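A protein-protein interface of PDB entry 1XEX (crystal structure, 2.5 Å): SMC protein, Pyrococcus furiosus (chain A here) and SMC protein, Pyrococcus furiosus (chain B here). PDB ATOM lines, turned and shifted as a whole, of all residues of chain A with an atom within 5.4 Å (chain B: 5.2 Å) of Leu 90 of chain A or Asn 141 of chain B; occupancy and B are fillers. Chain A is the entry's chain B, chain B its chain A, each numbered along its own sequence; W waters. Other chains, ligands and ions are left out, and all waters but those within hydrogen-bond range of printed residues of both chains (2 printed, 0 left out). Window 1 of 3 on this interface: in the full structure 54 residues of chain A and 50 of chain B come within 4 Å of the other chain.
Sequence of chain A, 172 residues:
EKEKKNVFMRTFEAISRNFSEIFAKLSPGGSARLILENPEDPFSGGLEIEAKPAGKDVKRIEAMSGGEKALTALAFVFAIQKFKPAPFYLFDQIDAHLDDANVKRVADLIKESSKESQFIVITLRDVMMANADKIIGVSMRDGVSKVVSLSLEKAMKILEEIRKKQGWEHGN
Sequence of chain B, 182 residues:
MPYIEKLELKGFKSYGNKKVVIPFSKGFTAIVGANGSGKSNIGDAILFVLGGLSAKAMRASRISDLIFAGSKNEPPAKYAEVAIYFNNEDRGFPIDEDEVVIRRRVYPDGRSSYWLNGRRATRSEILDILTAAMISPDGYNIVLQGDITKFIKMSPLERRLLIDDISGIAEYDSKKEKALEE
Water W2 bridges O of Gly 139 of chain B (2.6 Å) and OH of Tyr 89 of chain A (3.0 Å). Water W1 bridges O of Leu 144 of chain B (2.8 Å) and O of Asp 92 of chain A (3.0 Å).
Of the 9 printed residues of chain A, 9 touch a printed residue of chain B. Printed residues of chain A that touch a printed residue of chain B: Gln 81, Ala 86, Phe 88, Tyr 89, Leu 90, Phe 91, Asp 92, Ile 120 and Ile 122. Hydrophobic or aromatic side chains of chain B that line the printed part of chain A: Ile 31, Ile 46, Ile 142 and Val 143. Among the printed residues, 15 pairs touch across the chains.
O of Tyr 89 of chain A is in hydrogen-bond range of N of Ile 120 of chain A. The side-chain amide oxygen (OD1) of Asn 141 of chain B lies close to the backbone carbonyl oxygen (O) of Ser 136 of chain B. OH of Tyr 89 of chain A sits at hydrogen-bond distance from N of Ala 86 of chain A. O of Phe 91 of chain A sits at hydrogen-bond distance from N of Ile 122 of chain A, 2.7 Å away. The side-chain hydroxyl of Tyr 89 of chain A sits at hydrogen-bond distance from the backbone carbonyl oxygen of Gln 81 of chain A, 3.3 Å away. N of Phe 91 of chain A is in hydrogen-bond range of O of Ile 120 of chain A, 2.9 Å away.
Leu 90 of chain A touches four residues of chain B. Of chain A, only Ala 86 (3.4 Å), Phe 88 (3.0 Å), Tyr 89 (3.1 Å) and Leu 90 (2.9 Å) come within 4 Å of Asn 141 of chain B. Of the printed residues of chain B, Asp 92 of chain A touches Val 143 and Leu 144. Of the printed residues of chain B, Tyr 89 of chain A touches Asn 141. Of the printed residues of chain B, Ile 120 of chain A touches Ile 31 (3.7 Å). Gly 139 of chain B touches none of the printed residues of chain A. Ser 136 of chain B touches none of the printed residues of chain A. The nearest residue of chain A that does not touch Asn 141 of chain B is Gln 81 of chain A (4.2 Å). The nearest printed residue of chain B that does not touch Asp 92 of chain A is Gly 43 of chain B (6.1 Å).
N of Val 143 of chain B sits at hydrogen-bond distance from O of Leu 90 of chain A. The backbone carbonyl oxygen of Asn 141 of chain B lies within hydrogen-bond range of the backbone NH of Leu 90 of chain A (2.9 Å). ND2 of Asn 141 of chain B is in hydrogen-bond range of O of Phe 88 of chain A (3.0 Å). O of Tyr 140 of chain B lies within hydrogen-bond range of NE2 of Gln 81 of chain A (3.0 Å). The backbone NH of Asp 92 of chain A sits at hydrogen-bond distance from the backbone carbonyl oxygen of Val 143 of chain B, at 2.9 Å.
Among the printed residues, pairs that only touch across the chains: Gln 81 of chain A with Val 143 of chain B (3.96 Å), Ala 86 of chain A with Asn 141 of chain B (3.4 Å), Phe 88 of chain A with Ile 46 of chain B (3.99 Å), Tyr 89 of chain A with Asn 141 of chain B (3.1 Å), Leu 90 of chain A with Gly 43 of chain B (3.5 Å), Leu 90 of chain A with Ile 142 of chain B (3.5 Å), Phe 91 of chain A with Val 143 of chain B (3.6 Å), Asp 92 of chain A with Leu 144 of chain B (3.9 Å), Ile 120 of chain A with Ile 31 of chain B (3.7 Å) and Ile 122 of chain A with Ile 31 of chain B (3.5 Å).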
ATOM      1  N   GLN A  81      -7.091  20.817 -27.968  1.00  0.00           N
ATOM      2  CA  GLN A  81      -5.682  20.545 -28.233  1.00  0.00           C
ATOM      3  C   GLN A  81      -4.973  21.793 -28.756  1.00  0.00           C
ATOM      4  O   GLN A  81      -3.764  21.954 -28.572  1.00  0.00           O
ATOM      5  CB  GLN A  81      -5.542  19.405 -29.244  1.00  0.00           C
ATOM      6  CG  GLN A  81      -6.209  18.106 -28.815  1.00  0.00           C
ATOM      7  CD  GLN A  81      -6.183  17.044 -29.899  1.00  0.00           C
ATOM      8  OE1 GLN A  81      -6.264  17.347 -31.091  1.00  0.00           O
ATOM      9  NE2 GLN A  81      -6.072  15.785 -29.487  1.00  0.00           N
ATOM     10  N   ALA A  86       0.410  20.189 -27.907  1.00  0.00           N
ATOM     11  CA  ALA A  86       1.277  19.115 -27.441  1.00  0.00           C
ATOM     12  C   ALA A  86       2.346  18.814 -28.492  1.00  0.00           C
ATOM     13  O   ALA A  86       2.151  19.081 -29.679  1.00  0.00           O
ATOM     14  CB  ALA A  86       0.449  17.865 -27.153  1.00  0.00           C
ATOM     15  N   PHE A  88       3.232  16.021 -29.607  1.00  0.00           N
ATOM     16  CA  PHE A  88       2.778  14.914 -30.445  1.00  0.00           C
ATOM     17  C   PHE A  88       1.375  14.525 -30.044  1.00  0.00           C
ATOM     18  O   PHE A  88       0.924  14.848 -28.944  1.00  0.00           O
ATOM     19  CB  PHE A  88       3.727  13.719 -30.300  1.00  0.00           C
ATOM     20  CG  PHE A  88       3.481  12.871 -29.070  1.00  0.00           C
ATOM     21  CD1 PHE A  88       2.576  11.809 -29.110  1.00  0.00           C
ATOM     22  CD2 PHE A  88       4.174  13.126 -27.886  1.00  0.00           C
ATOM     23  CE1 PHE A  88       2.367  11.002 -27.984  1.00  0.00           C
ATOM     24  CE2 PHE A  88       3.976  12.332 -26.751  1.00  0.00           C
ATOM     25  CZ  PHE A  88       3.073  11.263 -26.793  1.00  0.00           C
ATOM     26  N   TYR A  89       0.681  13.859 -30.962  1.00  0.00           N
ATOM     27  CA  TYR A  89      -0.691  13.386 -30.727  1.00  0.00           C
ATOM     28  C   TYR A  89      -0.825  11.940 -31.176  1.00  0.00           C
ATOM     29  O   TYR A  89      -0.198  11.530 -32.146  1.00  0.00           O
ATOM     30  CB  TYR A  89      -1.693  14.230 -31.504  1.00  0.00           C
ATOM     31  CG  TYR A  89      -1.771  15.643 -31.031  1.00  0.00           C
ATOM     32  CD1 TYR A  89      -2.688  16.024 -30.066  1.00  0.00           C
ATOM     33  CD2 TYR A  89      -0.854  16.584 -31.478  1.00  0.00           C
ATOM     34  CE1 TYR A  89      -2.687  17.310 -29.552  1.00  0.00           C
ATOM     35  CE2 TYR A  89      -0.844  17.865 -30.971  1.00  0.00           C
ATOM     36  CZ  TYR A  89      -1.757  18.224 -30.017  1.00  0.00           C
ATOM     37  OH  TYR A  89      -1.752  19.520 -29.557  1.00  0.00           O
ATOM     38  N   LEU A  90      -1.612  11.163 -30.445  1.00  0.00           N
ATOM     39  CA  LEU A  90      -1.845   9.780 -30.812  1.00  0.00           C
ATOM     40  C   LEU A  90      -3.357   9.619 -30.931  1.00  0.00           C
ATOM     41  O   LEU A  90      -4.089   9.806 -29.966  1.00  0.00           O
ATOM     42  CB  LEU A  90      -1.310   8.830 -29.746  1.00  0.00           C
ATOM     43  CG  LEU A  90      -1.627   7.337 -29.934  1.00  0.00           C
ATOM     44  CD1 LEU A  90      -0.696   6.715 -30.959  1.00  0.00           C
ATOM     45  CD2 LEU A  90      -1.433   6.642 -28.600  1.00  0.00           C
ATOM     46  N   PHE A  91      -3.823   9.287 -32.124  1.00  0.00           N
ATOM     47  CA  PHE A  91      -5.246   9.115 -32.357  1.00  0.00           C
ATOM     48  C   PHE A  91      -5.550   7.664 -32.725  1.00  0.00           C
ATOM     49  O   PHE A  91      -4.968   7.124 -33.657  1.00  0.00           O
ATOM     50  CB  PHE A  91      -5.697  10.039 -33.489  1.00  0.00           C
ATOM     51  CG  PHE A  91      -5.494  11.500 -33.209  1.00  0.00           C
ATOM     52  CD1 PHE A  91      -5.264  12.392 -34.246  1.00  0.00           C
ATOM     53  CD2 PHE A  91      -5.595  12.004 -31.920  1.00  0.00           C
ATOM     54  CE1 PHE A  91      -5.143  13.763 -33.997  1.00  0.00           C
ATOM     55  CE2 PHE A  91      -5.474  13.394 -31.673  1.00  0.00           C
ATOM     56  CZ  PHE A  91      -5.252  14.258 -32.704  1.00  0.00           C
ATOM     57  N   ASP A  92      -6.451   7.029 -31.978  1.00  0.00           N
ATOM     58  CA  ASP A  92      -6.840   5.648 -32.263  1.00  0.00           C
ATOM     59  C   ASP A  92      -8.293   5.624 -32.760  1.00  0.00           C
ATOM     60  O   ASP A  92      -9.219   5.894 -31.999  1.00  0.00           O
ATOM     61  CB  ASP A  92      -6.722   4.785 -31.004  1.00  0.00           C
ATOM     62  CG  ASP A  92      -6.655   3.289 -31.316  1.00  0.00           C
ATOM     63  OD1 ASP A  92      -6.972   2.897 -32.458  1.00  0.00           O
ATOM     64  OD2 ASP A  92      -6.287   2.495 -30.416  1.00  0.00           O
ATOM     65  N   ILE A 120       0.396  10.740 -34.809  1.00  0.00           N
ATOM     66  CA  ILE A 120       0.414   9.288 -34.966  1.00  0.00           C
ATOM     67  C   ILE A 120      -1.031   8.795 -34.919  1.00  0.00           C
ATOM     68  O   ILE A 120      -1.616   8.657 -33.842  1.00  0.00           O
ATOM     69  CB  ILE A 120       1.222   8.599 -33.837  1.00  0.00           C
ATOM     70  CG1 ILE A 120       2.614   9.225 -33.719  1.00  0.00           C
ATOM     71  CG2 ILE A 120       1.337   7.102 -34.112  1.00  0.00           C
ATOM     72  CD1 ILE A 120       3.451   8.660 -32.587  1.00  0.00           C
ATOM     73  N   ILE A 122      -3.922   5.898 -35.773  1.00  0.00           N
ATOM     74  CA  ILE A 122      -4.187   4.485 -36.023  1.00  0.00           C
ATOM     75  C   ILE A 122      -5.594   4.386 -36.607  1.00  0.00           C
ATOM     76  O   ILE A 122      -6.582   4.600 -35.898  1.00  0.00           O
ATOM     77  CB  ILE A 122      -4.121   3.649 -34.722  1.00  0.00           C
ATOM     78  CG1 ILE A 122      -2.806   3.912 -33.983  1.00  0.00           C
ATOM     79  CG2 ILE A 122      -4.262   2.164 -35.041  1.00  0.00           C
ATOM     80  CD1 ILE A 122      -2.896   3.731 -32.480  1.00  0.00           C
ATOM     81  N   ILE B  31      -0.766   4.114 -38.635  1.00  0.00           N
ATOM     82  CA  ILE B  31      -0.524   2.745 -38.222  1.00  0.00           C
ATOM     83  C   ILE B  31      -1.732   1.958 -38.723  1.00  0.00           C
ATOM     84  O   ILE B  31      -2.865   2.249 -38.343  1.00  0.00           O
ATOM     85  CB  ILE B  31      -0.440   2.608 -36.665  1.00  0.00           C
ATOM     86  CG1 ILE B  31       0.794   3.362 -36.119  1.00  0.00           C
ATOM     87  CG2 ILE B  31      -0.362   1.137 -36.294  1.00  0.00           C
ATOM     88  CD1 ILE B  31       0.862   3.472 -34.578  1.00  0.00           C
ATOM     89  N   GLY B  43      -0.200   2.066 -28.934  1.00  0.00           N
ATOM     90  CA  GLY B  43      -0.656   3.241 -28.222  1.00  0.00           C
ATOM     91  C   GLY B  43      -0.456   2.970 -26.740  1.00  0.00           C
ATOM     92  O   GLY B  43       0.024   3.820 -25.983  1.00  0.00           O
ATOM     93  N   ILE B  46       2.950   3.593 -25.425  1.00  0.00           N
ATOM     94  CA  ILE B  46       3.282   4.996 -25.212  1.00  0.00           C
ATOM     95  C   ILE B  46       2.707   5.495 -23.891  1.00  0.00           C
ATOM     96  O   ILE B  46       3.385   6.194 -23.164  1.00  0.00           O
ATOM     97  CB  ILE B  46       2.768   5.863 -26.390  1.00  0.00           C
ATOM     98  CG1 ILE B  46       3.485   5.437 -27.670  1.00  0.00           C
ATOM     99  CG2 ILE B  46       2.986   7.336 -26.098  1.00  0.00           C
ATOM    100  CD1 ILE B  46       3.018   6.172 -28.908  1.00  0.00           C
ATOM    101  N   ILE B 135       4.083  17.829 -22.408  1.00  0.00           N
ATOM    102  CA  ILE B 135       3.559  16.488 -22.611  1.00  0.00           C
ATOM    103  C   ILE B 135       2.887  16.037 -21.322  1.00  0.00           C
ATOM    104  O   ILE B 135       3.546  15.569 -20.402  1.00  0.00           O
ATOM    105  CB  ILE B 135       4.673  15.479 -22.944  1.00  0.00           C
ATOM    106  CG1 ILE B 135       5.339  15.855 -24.267  1.00  0.00           C
ATOM    107  CG2 ILE B 135       4.092  14.071 -22.993  1.00  0.00           C
ATOM    108  CD1 ILE B 135       6.538  15.015 -24.612  1.00  0.00           C
ATOM    109  N   SER B 136       1.568  16.170 -21.251  1.00  0.00           N
ATOM    110  CA  SER B 136       0.851  15.785 -20.042  1.00  0.00           C
ATOM    111  C   SER B 136      -0.504  15.185 -20.341  1.00  0.00           C
ATOM    112  O   SER B 136      -1.023  15.320 -21.443  1.00  0.00           O
ATOM    113  CB  SER B 136       0.644  17.010 -19.149  1.00  0.00           C
ATOM    114  OG  SER B 136      -0.260  17.923 -19.757  1.00  0.00           O
ATOM    115  N   GLY B 139      -3.117  17.505 -21.442  1.00  0.00           N
ATOM    116  CA  GLY B 139      -2.962  18.089 -22.763  1.00  0.00           C
ATOM    117  C   GLY B 139      -3.936  17.442 -23.736  1.00  0.00           C
ATOM    118  O   GLY B 139      -4.176  17.964 -24.830  1.00  0.00           O
ATOM    119  N   TYR B 140      -4.499  16.300 -23.333  1.00  0.00           N
ATOM    120  CA  TYR B 140      -5.456  15.575 -24.162  1.00  0.00           C
ATOM    121  C   TYR B 140      -4.887  15.321 -25.546  1.00  0.00           C
ATOM    122  O   TYR B 140      -5.587  15.458 -26.543  1.00  0.00           O
ATOM    123  CB  TYR B 140      -6.745  16.385 -24.295  1.00  0.00           C
ATOM    124  CG  TYR B 140      -7.388  16.663 -22.970  1.00  0.00           C
ATOM    125  CD1 TYR B 140      -7.367  17.942 -22.412  1.00  0.00           C
ATOM    126  CD2 TYR B 140      -7.980  15.627 -22.243  1.00  0.00           C
ATOM    127  CE1 TYR B 140      -7.922  18.183 -21.147  1.00  0.00           C
ATOM    128  CE2 TYR B 140      -8.535  15.851 -20.981  1.00  0.00           C
ATOM    129  CZ  TYR B 140      -8.505  17.127 -20.435  1.00  0.00           C
ATOM    130  OH  TYR B 140      -9.046  17.336 -19.178  1.00  0.00           O
ATOM    131  N   ASN B 141      -3.616  14.954 -25.609  1.00  0.00           N
ATOM    132  CA  ASN B 141      -2.988  14.725 -26.889  1.00  0.00           C
ATOM    133  C   ASN B 141      -3.125  13.271 -27.317  1.00  0.00           C
ATOM    134  O   ASN B 141      -2.708  12.891 -28.412  1.00  0.00           O
ATOM    135  CB  ASN B 141      -1.517  15.126 -26.820  1.00  0.00           C
ATOM    136  CG  ASN B 141      -0.749  14.312 -25.812  1.00  0.00           C
ATOM    137  OD1 ASN B 141      -1.205  14.133 -24.679  1.00  0.00           O
ATOM    138  ND2 ASN B 141       0.423  13.810 -26.210  1.00  0.00           N
ATOM    139  N   ILE B 142      -3.709  12.462 -26.445  1.00  0.00           N
ATOM    140  CA  ILE B 142      -3.913  11.051 -26.725  1.00  0.00           C
ATOM    141  C   ILE B 142      -5.410  10.717 -26.689  1.00  0.00           C
ATOM    142  O   ILE B 142      -6.066  10.831 -25.658  1.00  0.00           O
ATOM    143  CB  ILE B 142      -3.108  10.186 -25.724  1.00  0.00           C
ATOM    144  CG1 ILE B 142      -1.616  10.521 -25.858  1.00  0.00           C
ATOM    145  CG2 ILE B 142      -3.337   8.709 -25.990  1.00  0.00           C
ATOM    146  CD1 ILE B 142      -0.688   9.623 -25.082  1.00  0.00           C
ATOM    147  N   VAL B 143      -5.944  10.337 -27.845  1.00  0.00           N
ATOM    148  CA  VAL B 143      -7.356   9.991 -27.999  1.00  0.00           C
ATOM    149  C   VAL B 143      -7.452   8.491 -28.267  1.00  0.00           C
ATOM    150  O   VAL B 143      -7.168   8.032 -29.376  1.00  0.00           O
ATOM    151  CB  VAL B 143      -7.985  10.747 -29.190  1.00  0.00           C
ATOM    152  CG1 VAL B 143      -9.440  10.419 -29.301  1.00  0.00           C
ATOM    153  CG2 VAL B 143      -7.777  12.244 -29.026  1.00  0.00           C
ATOM    154  N   LEU B 144      -7.866   7.741 -27.251  1.00  0.00           N
ATOM    155  CA  LEU B 144      -7.975   6.284 -27.335  1.00  0.00           C
ATOM    156  C   LEU B 144      -9.184   5.747 -28.099  1.00  0.00           C
ATOM    157  O   LEU B 144     -10.189   6.439 -28.279  1.00  0.00           O
ATOM    158  CB  LEU B 144      -7.983   5.689 -25.927  1.00  0.00           C
ATOM    159  CG  LEU B 144      -6.664   5.448 -25.179  1.00  0.00           C
ATOM    160  CD1 LEU B 144      -5.599   6.436 -25.617  1.00  0.00           C
ATOM    161  CD2 LEU B 144      -6.921   5.529 -23.666  1.00  0.00           C
HETATM  162  O   HOH W   1     -11.515   7.193 -30.570  1.00  0.00           O
HETATM  163  O   HOH W   2      -2.864  18.765 -26.886  1.00  0.00           O
